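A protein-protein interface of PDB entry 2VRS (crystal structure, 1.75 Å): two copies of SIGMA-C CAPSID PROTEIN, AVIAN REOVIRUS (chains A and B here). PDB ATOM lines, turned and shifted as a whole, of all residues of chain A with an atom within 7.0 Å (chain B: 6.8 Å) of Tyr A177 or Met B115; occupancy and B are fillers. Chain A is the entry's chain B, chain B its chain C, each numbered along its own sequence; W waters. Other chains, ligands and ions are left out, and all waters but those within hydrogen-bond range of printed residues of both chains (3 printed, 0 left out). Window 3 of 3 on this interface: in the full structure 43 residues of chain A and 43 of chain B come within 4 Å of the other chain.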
ATOM      1  N   SER A 158      -6.811 -21.877 -14.279  1.00  0.00           N
ATOM      2  CA  SER A 158      -8.012 -22.492 -13.687  1.00  0.00           C
ATOM      3  C   SER A 158      -9.204 -21.530 -13.855  1.00  0.00           C
ATOM      4  O   SER A 158      -9.033 -20.304 -14.022  1.00  0.00           O
ATOM      5  CB  SER A 158      -7.779 -22.817 -12.210  1.00  0.00           C
ATOM      6  OG  SER A 158      -6.823 -23.880 -12.131  1.00  0.00           O
ATOM      7  N   PHE A 159     -10.403 -22.096 -13.891  1.00  0.00           N
ATOM      8  CA  PHE A 159     -11.635 -21.263 -14.103  1.00  0.00           C
ATOM      9  C   PHE A 159     -12.768 -21.763 -13.184  1.00  0.00           C
ATOM     10  O   PHE A 159     -12.796 -22.952 -12.807  1.00  0.00           O
ATOM     11  CB  PHE A 159     -12.096 -21.321 -15.586  1.00  0.00           C
ATOM     12  CG  PHE A 159     -12.307 -22.754 -16.117  1.00  0.00           C
ATOM     13  CD1 PHE A 159     -11.226 -23.486 -16.644  1.00  0.00           C
ATOM     14  CD2 PHE A 159     -13.597 -23.367 -16.071  1.00  0.00           C
ATOM     15  CE1 PHE A 159     -11.414 -24.826 -17.140  1.00  0.00           C
ATOM     16  CE2 PHE A 159     -13.813 -24.679 -16.557  1.00  0.00           C
ATOM     17  CZ  PHE A 159     -12.710 -25.427 -17.086  1.00  0.00           C
ATOM     18  N   PRO A 160     -13.640 -20.849 -12.750  1.00  0.00           N
ATOM     19  CA  PRO A 160     -14.713 -21.208 -11.778  1.00  0.00           C
ATOM     20  C   PRO A 160     -15.757 -22.152 -12.374  1.00  0.00           C
ATOM     21  O   PRO A 160     -16.091 -22.047 -13.553  1.00  0.00           O
ATOM     22  CB  PRO A 160     -15.326 -19.845 -11.392  1.00  0.00           C
ATOM     23  CG  PRO A 160     -14.905 -18.894 -12.506  1.00  0.00           C
ATOM     24  CD  PRO A 160     -13.632 -19.412 -13.102  1.00  0.00           C
ATOM     25  N   VAL A 161     -16.211 -23.115 -11.553  1.00  0.00           N
ATOM     26  CA  VAL A 161     -17.233 -24.131 -11.912  1.00  0.00           C
ATOM     27  C   VAL A 161     -18.145 -24.170 -10.669  1.00  0.00           C
ATOM     28  O   VAL A 161     -17.649 -24.276  -9.542  1.00  0.00           O
ATOM     29  CB  VAL A 161     -16.559 -25.554 -12.098  1.00  0.00           C
ATOM     30  CG1 VAL A 161     -17.645 -26.614 -12.284  1.00  0.00           C
ATOM     31  CG2 VAL A 161     -15.589 -25.520 -13.267  1.00  0.00           C
ATOM     32  N   ASP A 162     -19.456 -24.019 -10.832  1.00  0.00           N
ATOM     33  CA  ASP A 162     -20.378 -24.302  -9.703  1.00  0.00           C
ATOM     34  C   ASP A 162     -20.847 -25.745  -9.767  1.00  0.00           C
ATOM     35  O   ASP A 162     -21.278 -26.195 -10.817  1.00  0.00           O
ATOM     36  CB  ASP A 162     -21.623 -23.399  -9.850  1.00  0.00           C
ATOM     37  CG  ASP A 162     -21.287 -21.911  -9.835  1.00  0.00           C
ATOM     38  OD1 ASP A 162     -20.431 -21.482  -9.049  1.00  0.00           O
ATOM     39  OD2 ASP A 162     -21.913 -21.171 -10.606  1.00  0.00           O
ATOM     40  N   VAL A 163     -20.812 -26.457  -8.636  1.00  0.00           N
ATOM     41  CA  VAL A 163     -21.378 -27.807  -8.584  1.00  0.00           C
ATOM     42  C   VAL A 163     -22.433 -27.918  -7.477  1.00  0.00           C
ATOM     43  O   VAL A 163     -22.360 -27.194  -6.468  1.00  0.00           O
ATOM     44  CB  VAL A 163     -20.287 -28.880  -8.399  1.00  0.00           C
ATOM     45  CG1 VAL A 163     -19.200 -28.773  -9.497  1.00  0.00           C
ATOM     46  CG2 VAL A 163     -19.653 -28.849  -6.998  1.00  0.00           C
ATOM     47  N   TYR A 174     -20.994 -26.116  -4.037  1.00  0.00           N
ATOM     48  CA  TYR A 174     -19.657 -25.566  -3.833  1.00  0.00           C
ATOM     49  C   TYR A 174     -19.293 -24.726  -5.030  1.00  0.00           C
ATOM     50  O   TYR A 174     -19.730 -24.976  -6.150  1.00  0.00           O
ATOM     51  CB  TYR A 174     -18.601 -26.656  -3.641  1.00  0.00           C
ATOM     52  CG  TYR A 174     -18.894 -27.527  -2.437  1.00  0.00           C
ATOM     53  CD1 TYR A 174     -18.667 -27.058  -1.142  1.00  0.00           C
ATOM     54  CD2 TYR A 174     -19.466 -28.798  -2.588  1.00  0.00           C
ATOM     55  CE1 TYR A 174     -18.970 -27.835  -0.034  1.00  0.00           C
ATOM     56  CE2 TYR A 174     -19.782 -29.600  -1.470  1.00  0.00           C
ATOM     57  CZ  TYR A 174     -19.519 -29.112  -0.194  1.00  0.00           C
ATOM     58  OH  TYR A 174     -19.822 -29.872   0.932  1.00  0.00           O
ATOM     59  N   GLN A 175     -18.521 -23.698  -4.761  1.00  0.00           N
ATOM     60  CA  GLN A 175     -17.876 -22.937  -5.807  1.00  0.00           C
ATOM     61  C   GLN A 175     -16.556 -23.639  -5.952  1.00  0.00           C
ATOM     62  O   GLN A 175     -15.767 -23.654  -4.999  1.00  0.00           O
ATOM     63  CB  GLN A 175     -17.590 -21.528  -5.283  1.00  0.00           C
ATOM     64  CG  GLN A 175     -16.581 -20.768  -6.119  1.00  0.00           C
ATOM     65  CD  GLN A 175     -17.175 -20.406  -7.415  1.00  0.00           C
ATOM     66  OE1 GLN A 175     -18.080 -19.579  -7.474  1.00  0.00           O
ATOM     67  NE2 GLN A 175     -16.690 -21.019  -8.479  1.00  0.00           N
ATOM     68  N   ALA A 176     -16.317 -24.231  -7.133  1.00  0.00           N
ATOM     69  CA  ALA A 176     -15.188 -25.096  -7.374  1.00  0.00           C
ATOM     70  C   ALA A 176     -14.464 -24.567  -8.626  1.00  0.00           C
ATOM     71  O   ALA A 176     -14.791 -23.484  -9.111  1.00  0.00           O
ATOM     72  CB  ALA A 176     -15.679 -26.542  -7.585  1.00  0.00           C
ATOM     73  N   TYR A 177     -13.460 -25.298  -9.089  1.00  0.00           N
ATOM     74  CA  TYR A 177     -12.588 -24.845 -10.187  1.00  0.00           C
ATOM     75  C   TYR A 177     -12.301 -25.996 -11.134  1.00  0.00           C
ATOM     76  O   TYR A 177     -12.284 -27.190 -10.718  1.00  0.00           O
ATOM     77  CB  TYR A 177     -11.294 -24.160  -9.663  1.00  0.00           C
ATOM     78  CG  TYR A 177     -11.641 -22.838  -8.988  1.00  0.00           C
ATOM     79  CD1 TYR A 177     -12.064 -22.813  -7.647  1.00  0.00           C
ATOM     80  CD2 TYR A 177     -11.633 -21.625  -9.696  1.00  0.00           C
ATOM     81  CE1 TYR A 177     -12.458 -21.645  -7.032  1.00  0.00           C
ATOM     82  CE2 TYR A 177     -12.010 -20.428  -9.066  1.00  0.00           C
ATOM     83  CZ  TYR A 177     -12.425 -20.454  -7.728  1.00  0.00           C
ATOM     84  OH  TYR A 177     -12.847 -19.307  -7.059  1.00  0.00           O
ATOM     85  N   GLY A 178     -12.098 -25.644 -12.398  1.00  0.00           N
ATOM     86  CA  GLY A 178     -11.661 -26.610 -13.429  1.00  0.00           C
ATOM     87  C   GLY A 178     -10.369 -26.103 -14.043  1.00  0.00           C
ATOM     88  O   GLY A 178      -9.988 -24.900 -13.890  1.00  0.00           O
ATOM     89  N   VAL A 179      -9.694 -27.000 -14.751  1.00  0.00           N
ATOM     90  CA  VAL A 179      -8.495 -26.644 -15.496  1.00  0.00           C
ATOM     91  C   VAL A 179      -8.395 -27.591 -16.681  1.00  0.00           C
ATOM     92  O   VAL A 179      -8.655 -28.795 -16.522  1.00  0.00           O
ATOM     93  CB  VAL A 179      -7.193 -26.722 -14.574  1.00  0.00           C
ATOM     94  CG1 VAL A 179      -6.919 -28.132 -14.124  1.00  0.00           C
ATOM     95  CG2 VAL A 179      -5.951 -26.189 -15.327  1.00  0.00           C
ATOM     96  N   THR A 187     -10.587 -30.991 -16.169  1.00  0.00           N
ATOM     97  CA  THR A 187     -10.963 -31.701 -14.947  1.00  0.00           C
ATOM     98  C   THR A 187     -11.454 -30.690 -13.945  1.00  0.00           C
ATOM     99  O   THR A 187     -10.825 -29.628 -13.749  1.00  0.00           O
ATOM    100  CB  THR A 187      -9.751 -32.526 -14.375  1.00  0.00           C
ATOM    101  OG1 THR A 187      -9.370 -33.507 -15.345  1.00  0.00           O
ATOM    102  CG2 THR A 187     -10.115 -33.202 -13.043  1.00  0.00           C
ATOM    103  N   ILE A 188     -12.582 -31.001 -13.329  1.00  0.00           N
ATOM    104  CA  ILE A 188     -13.076 -30.206 -12.208  1.00  0.00           C
ATOM    105  C   ILE A 188     -12.690 -30.864 -10.879  1.00  0.00           C
ATOM    106  O   ILE A 188     -12.649 -32.096 -10.775  1.00  0.00           O
ATOM    107  CB  ILE A 188     -14.598 -29.845 -12.336  1.00  0.00           C
ATOM    108  CG1 ILE A 188     -15.486 -31.076 -12.259  1.00  0.00           C
ATOM    109  CG2 ILE A 188     -14.817 -29.171 -13.706  1.00  0.00           C
ATOM    110  CD1 ILE A 188     -17.000 -30.741 -12.338  1.00  0.00           C
ATOM    111  N   THR A 189     -12.353 -30.029  -9.907  1.00  0.00           N
ATOM    112  CA  THR A 189     -11.984 -30.502  -8.546  1.00  0.00           C
ATOM    113  C   THR A 189     -13.038 -29.937  -7.586  1.00  0.00           C
ATOM    114  O   THR A 189     -13.295 -28.724  -7.568  1.00  0.00           O
ATOM    115  CB  THR A 189     -10.539 -30.042  -8.176  1.00  0.00           C
ATOM    116  OG1 THR A 189      -9.587 -30.650  -9.067  1.00  0.00           O
ATOM    117  CG2 THR A 189     -10.178 -30.428  -6.728  1.00  0.00           C
ATOM    118  N   PHE A 190     -13.697 -30.800  -6.802  1.00  0.00           N
ATOM    119  CA  PHE A 190     -14.694 -30.282  -5.875  1.00  0.00           C
ATOM    120  C   PHE A 190     -14.847 -31.135  -4.609  1.00  0.00           C
ATOM    121  O   PHE A 190     -14.475 -32.321  -4.645  1.00  0.00           O
ATOM    122  CB  PHE A 190     -16.043 -30.030  -6.576  1.00  0.00           C
ATOM    123  CG  PHE A 190     -16.706 -31.282  -7.171  1.00  0.00           C
ATOM    124  CD1 PHE A 190     -16.389 -31.711  -8.471  1.00  0.00           C
ATOM    125  CD2 PHE A 190     -17.658 -32.019  -6.423  1.00  0.00           C
ATOM    126  CE1 PHE A 190     -16.993 -32.857  -9.035  1.00  0.00           C
ATOM    127  CE2 PHE A 190     -18.295 -33.150  -6.986  1.00  0.00           C
ATOM    128  CZ  PHE A 190     -17.962 -33.559  -8.306  1.00  0.00           C
ATOM    129  N   LEU B  82      -5.859 -16.758 -12.734  1.00  0.00           N
ATOM    130  CA  LEU B  82      -6.682 -16.866 -11.559  1.00  0.00           C
ATOM    131  C   LEU B  82      -5.842 -16.294 -10.411  1.00  0.00           C
ATOM    132  O   LEU B  82      -4.939 -16.966  -9.879  1.00  0.00           O
ATOM    133  CB  LEU B  82      -7.091 -18.339 -11.270  1.00  0.00           C
ATOM    134  CG  LEU B  82      -8.118 -18.493 -10.107  1.00  0.00           C
ATOM    135  CD1 LEU B  82      -9.526 -17.861 -10.451  1.00  0.00           C
ATOM    136  CD2 LEU B  82      -8.323 -19.944  -9.732  1.00  0.00           C
ATOM    137  N   THR B 102     -11.354 -13.691   1.480  1.00  0.00           N
ATOM    138  CA  THR B 102     -10.498 -14.438   0.582  1.00  0.00           C
ATOM    139  C   THR B 102     -11.060 -14.322  -0.838  1.00  0.00           C
ATOM    140  O   THR B 102     -12.225 -14.656  -1.100  1.00  0.00           O
ATOM    141  CB  THR B 102     -10.461 -15.909   1.033  1.00  0.00           C
ATOM    142  OG1 THR B 102      -9.866 -15.930   2.347  1.00  0.00           O
ATOM    143  CG2 THR B 102      -9.676 -16.789   0.075  1.00  0.00           C
ATOM    144  N   VAL B 103     -10.234 -13.806  -1.735  1.00  0.00           N
ATOM    145  CA  VAL B 103     -10.734 -13.436  -3.086  1.00  0.00           C
ATOM    146  C   VAL B 103     -10.037 -14.266  -4.144  1.00  0.00           C
ATOM    147  O   VAL B 103      -8.816 -14.387  -4.145  1.00  0.00           O
ATOM    148  CB  VAL B 103     -10.489 -11.937  -3.432  1.00  0.00           C
ATOM    149  CG1 VAL B 103     -10.977 -11.644  -4.871  1.00  0.00           C
ATOM    150  CG2 VAL B 103     -11.169 -10.995  -2.402  1.00  0.00           C
ATOM    151  N   ASN B 104     -10.824 -14.841  -5.059  1.00  0.00           N
ATOM    152  CA  ASN B 104     -10.297 -15.349  -6.307  1.00  0.00           C
ATOM    153  C   ASN B 104     -10.838 -14.477  -7.440  1.00  0.00           C
ATOM    154  O   ASN B 104     -12.035 -14.322  -7.544  1.00  0.00           O
ATOM    155  CB  ASN B 104     -10.789 -16.764  -6.559  1.00  0.00           C
ATOM    156  CG  ASN B 104     -10.029 -17.791  -5.750  1.00  0.00           C
ATOM    157  OD1 ASN B 104      -8.996 -18.292  -6.181  1.00  0.00           O
ATOM    158  ND2 ASN B 104     -10.546 -18.126  -4.609  1.00  0.00           N
ATOM    159  N   ALA B 105      -9.932 -13.919  -8.229  1.00  0.00           N
ATOM    160  CA  ALA B 105     -10.261 -13.065  -9.351  1.00  0.00           C
ATOM    161  C   ALA B 105      -9.864 -13.796 -10.628  1.00  0.00           C
ATOM    162  O   ALA B 105      -8.679 -14.073 -10.881  1.00  0.00           O
ATOM    163  CB  ALA B 105      -9.521 -11.661  -9.195  1.00  0.00           C
ATOM    164  N   HIS B 106     -10.870 -14.180 -11.406  1.00  0.00           N
ATOM    165  CA  HIS B 106     -10.615 -14.894 -12.644  1.00  0.00           C
ATOM    166  C   HIS B 106     -10.596 -13.899 -13.777  1.00  0.00           C
ATOM    167  O   HIS B 106     -11.642 -13.317 -14.131  1.00  0.00           O
ATOM    168  CB  HIS B 106     -11.696 -15.983 -12.871  1.00  0.00           C
ATOM    169  CG  HIS B 106     -11.487 -16.781 -14.124  1.00  0.00           C
ATOM    170  ND1 HIS B 106     -12.476 -16.960 -15.065  1.00  0.00           N
ATOM    171  CD2 HIS B 106     -10.397 -17.440 -14.591  1.00  0.00           C
ATOM    172  CE1 HIS B 106     -12.006 -17.689 -16.064  1.00  0.00           C
ATOM    173  NE2 HIS B 106     -10.753 -18.008 -15.793  1.00  0.00           N
ATOM    174  N   ASP B 113     -13.716 -11.661 -13.035  1.00  0.00           N
ATOM    175  CA  ASP B 113     -14.825 -12.163 -12.195  1.00  0.00           C
ATOM    176  C   ASP B 113     -14.335 -12.444 -10.822  1.00  0.00           C
ATOM    177  O   ASP B 113     -13.344 -13.159 -10.672  1.00  0.00           O
ATOM    178  CB  ASP B 113     -15.481 -13.399 -12.841  1.00  0.00           C
ATOM    179  CG  ASP B 113     -16.162 -13.042 -14.184  1.00  0.00           C
ATOM    180  OD1 ASP B 113     -16.940 -12.063 -14.174  1.00  0.00           O
ATOM    181  OD2 ASP B 113     -15.916 -13.714 -15.204  1.00  0.00           O
ATOM    182  N   TYR B 114     -14.992 -11.833  -9.824  1.00  0.00           N
ATOM    183  CA  TYR B 114     -14.603 -12.000  -8.425  1.00  0.00           C
ATOM    184  C   TYR B 114     -15.442 -13.059  -7.729  1.00  0.00           C
ATOM    185  O   TYR B 114     -16.670 -13.058  -7.799  1.00  0.00           O
ATOM    186  CB  TYR B 114     -14.839 -10.688  -7.665  1.00  0.00           C
ATOM    187  CG  TYR B 114     -13.874  -9.581  -7.947  1.00  0.00           C
ATOM    188  CD1 TYR B 114     -12.498  -9.781  -7.896  1.00  0.00           C
ATOM    189  CD2 TYR B 114     -14.355  -8.282  -8.174  1.00  0.00           C
ATOM    190  CE1 TYR B 114     -11.584  -8.697  -8.103  1.00  0.00           C
ATOM    191  CE2 TYR B 114     -13.485  -7.232  -8.354  1.00  0.00           C
ATOM    192  CZ  TYR B 114     -12.110  -7.426  -8.333  1.00  0.00           C
ATOM    193  OH  TYR B 114     -11.285  -6.333  -8.516  1.00  0.00           O
ATOM    194  N   MET B 115     -14.759 -13.956  -7.013  1.00  0.00           N
ATOM    195  CA  MET B 115     -15.446 -14.882  -6.138  1.00  0.00           C
ATOM    196  C   MET B 115     -14.810 -14.681  -4.759  1.00  0.00           C
ATOM    197  O   MET B 115     -13.623 -14.927  -4.614  1.00  0.00           O
ATOM    198  CB  MET B 115     -15.196 -16.325  -6.647  1.00  0.00           C
ATOM    199  CG  MET B 115     -16.050 -16.713  -7.828  1.00  0.00           C
ATOM    200  SD  MET B 115     -15.556 -16.091  -9.483  1.00  0.00           S
ATOM    201  CE  MET B 115     -13.791 -16.422  -9.580  1.00  0.00           C
ATOM    202  N   MET B 116     -15.590 -14.252  -3.766  1.00  0.00           N
ATOM    203  CA  MET B 116     -15.028 -13.941  -2.425  1.00  0.00           C
ATOM    204  C   MET B 116     -15.771 -14.671  -1.324  1.00  0.00           C
ATOM    205  O   MET B 116     -17.006 -14.841  -1.377  1.00  0.00           O
ATOM    206  CB  MET B 116     -15.223 -12.469  -2.130  1.00  0.00           C
ATOM    207  CG  MET B 116     -14.726 -11.542  -3.252  1.00  0.00           C
ATOM    208  SD  MET B 116     -14.880  -9.823  -2.668  1.00  0.00           S
ATOM    209  CE  MET B 116     -14.614  -8.902  -4.160  1.00  0.00           C
ATOM    210  N   SER B 117     -15.014 -15.088  -0.309  1.00  0.00           N
ATOM    211  CA  SER B 117     -15.644 -15.689   0.846  1.00  0.00           C
ATOM    212  C   SER B 117     -14.945 -15.192   2.104  1.00  0.00           C
ATOM    213  O   SER B 117     -13.775 -14.791   2.082  1.00  0.00           O
ATOM    214  CB  SER B 117     -15.606 -17.222   0.761  1.00  0.00           C
ATOM    215  OG  SER B 117     -14.282 -17.682   0.749  1.00  0.00           O
ATOM    216  N   THR B 204     -20.331 -14.276   1.337  1.00  0.00           N
ATOM    217  CA  THR B 204     -19.749 -14.545   0.030  1.00  0.00           C
ATOM    218  C   THR B 204     -20.195 -13.381  -0.867  1.00  0.00           C
ATOM    219  O   THR B 204     -21.278 -12.794  -0.674  1.00  0.00           O
ATOM    220  CB  THR B 204     -20.249 -15.897  -0.604  1.00  0.00           C
ATOM    221  OG1 THR B 204     -21.647 -15.786  -0.858  1.00  0.00           O
ATOM    222  CG2 THR B 204     -19.965 -17.102   0.322  1.00  0.00           C
ATOM    223  N   VAL B 205     -19.309 -12.981  -1.769  1.00  0.00           N
ATOM    224  CA  VAL B 205     -19.615 -11.878  -2.702  1.00  0.00           C
ATOM    225  C   VAL B 205     -19.191 -12.424  -4.079  1.00  0.00           C
ATOM    226  O   VAL B 205     -18.079 -12.961  -4.234  1.00  0.00           O
ATOM    227  CB  VAL B 205     -18.769 -10.609  -2.376  1.00  0.00           C
ATOM    228  CG1 VAL B 205     -18.931  -9.560  -3.468  1.00  0.00           C
ATOM    229  CG2 VAL B 205     -19.191  -9.965  -1.024  1.00  0.00           C
ATOM    230  N   ARG B 206     -20.092 -12.351  -5.046  1.00  0.00           N
ATOM    231  CA  ARG B 206     -19.784 -12.739  -6.426  1.00  0.00           C
ATOM    232  C   ARG B 206     -20.237 -11.615  -7.350  1.00  0.00           C
ATOM    233  O   ARG B 206     -21.396 -11.162  -7.291  1.00  0.00           O
ATOM    234  CB  ARG B 206     -20.492 -14.038  -6.814  1.00  0.00           C
ATOM    235  CG  ARG B 206     -20.089 -15.193  -5.944  1.00  0.00           C
ATOM    236  CD  ARG B 206     -20.395 -16.511  -6.623  1.00  0.00           C
ATOM    237  NE  ARG B 206     -19.792 -16.611  -7.956  1.00  0.00           N
ATOM    238  CZ  ARG B 206     -19.929 -17.675  -8.742  1.00  0.00           C
ATOM    239  NH1 ARG B 206     -20.638 -18.708  -8.319  1.00  0.00           N
ATOM    240  NH2 ARG B 206     -19.359 -17.715  -9.937  1.00  0.00           N
ATOM    241  N   THR B 207     -19.302 -11.185  -8.177  1.00  0.00           N
ATOM    242  CA  THR B 207     -19.571 -10.127  -9.138  1.00  0.00           C
ATOM    243  C   THR B 207     -18.494 -10.184 -10.214  1.00  0.00           C
ATOM    244  O   THR B 207     -17.607 -11.022 -10.183  1.00  0.00           O
ATOM    245  CB  THR B 207     -19.686  -8.713  -8.443  1.00  0.00           C
ATOM    246  OG1 THR B 207     -20.221  -7.761  -9.396  1.00  0.00           O
ATOM    247  CG2 THR B 207     -18.325  -8.197  -7.903  1.00  0.00           C
HETATM  248  O   HOH W   1      -9.262 -19.810 -17.423  1.00  0.00           O
HETATM  249  O   HOH W   2     -18.374 -20.433 -10.452  1.00  0.00           O
HETATM  250  O   HOH W   3     -13.694 -19.417  -4.510  1.00  0.00           O
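A ring nitrogen (NE2) of His B106 sits close to the backbone carbonyl oxygen (O) of Ser A158.
OD1 of Asp A162 lies within salt-bridge range of NH1 of Arg B206, 2.9 Å away.
The side-chain amide oxygen (OE1) of Gln A175 is in hydrogen-bond range of the guanidinium group (NH1) of Arg B206.
O of Phe A159 is in hydrogen-bond range of N of Gly A178 (2.8 Å).
The side-chain carboxylate (OD1) of Asp A162 lies close to the side-chain amide oxygen (OE1) of Gln A175.
The backbone NH (N) of Thr A189 sits at hydrogen-bond distance from the backbone carbonyl oxygen (O) of Tyr A177 (3.0 Å).
The backbone NH (N) of Met B115 is in hydrogen-bond range of the backbone carbonyl oxygen (O) of Asn B104, at 2.8 Å.
O of Asp B113 is in hydrogen-bond range of N of His B106, at 2.8 Å.
Ser A158 touches Leu B82.
His B106 touches Phe A159.
Pro A160 touches His B106 (CD to ND1, 3.3 Å).
CG of Pro A160 touches CE of Met B115, at 3.99 Å.
CG of Met B115 touches OE1 of Gln A175, at 3.5 Å.
Tyr A177 touches Leu B82 (CD2 to CD2, 3.7 Å).
OH of Tyr A177 touches CB of Asn B104, at 3.3 Å.
Met B115 touches Tyr A177 (CB to OH, 3.8 Å).
Printed residues of chain B within 4 Å of Gln A175: Met B115 (3.5 Å) and Arg B206 (2.8 Å).
Of chain B, only Leu B82 (3.7 Å), Asn B104 (3.3 Å) and Met B115 (3.8 Å) come within 4 Å of Tyr A177.
Thr B102 touches none of the printed residues of chain A.
Val B103 touches none of the printed residues of chain A.
Of the printed residues of chain A, His B106 touches Ser A158 (3.2 Å), Phe A159 (3.6 Å) and Pro A160 (3.3 Å).
Printed residues of chain A within 4 Å of Met B115: Pro A160, Gln A175 and Tyr A177.
Printed residues of chain A within 4 Å of Arg B206: Asp A162 and Gln A175.
The nearest residue of chain B that does not touch Tyr A177 is His B106 (5.9 Å).
The nearest printed residue of chain A that does not touch Asn B104 is Gln A175 (6.8 Å).
Of the 16 printed residues of chain A, 6 touch a printed residue of chain B.
Printed residues of chain A that touch a printed residue of chain B: Ser A158, Phe A159, Pro A160, Asp A162, Gln A175 and Tyr A177.
Hydrophobic or aromatic side chains of chain A within 4 Å of the printed part of chain B: Phe A159, Pro A160 and Tyr A177.
Of the 15 printed residues of chain B, 5 touch a printed residue of chain A.
Printed residues of chain B that touch a printed residue of chain A: Leu B82, Asn B104, His B106, Met B115 and Arg B206.
Hydrophobic or aromatic side chains of chain B within 4 Å of the printed part of chain A: Leu B82, His B106 and Met B115.
Among the printed residues, 11 pairs touch across the chains.
No position is printed for both chains.
Of the 11 pairs that touch across the chains among the printed residues, none has its exchanged pair printed and touching as well.
Water W2 lies within hydrogen-bond range of the side-chain amide nitrogen (NE2) of Gln A175, the side-chain carboxylate (OD1) of Asp A162 and the guanidinium group (NH2) of Arg B206.
Water W3 bridges OH of Tyr A177 (2.7 Å) and ND2 of Asn B104 (3.4 Å).
Water W1 lies within hydrogen-bond range of a ring nitrogen (NE2) of His B106 (2.9 Å) and the backbone carbonyl oxygen (O) of Ser A158 (3.4 Å).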
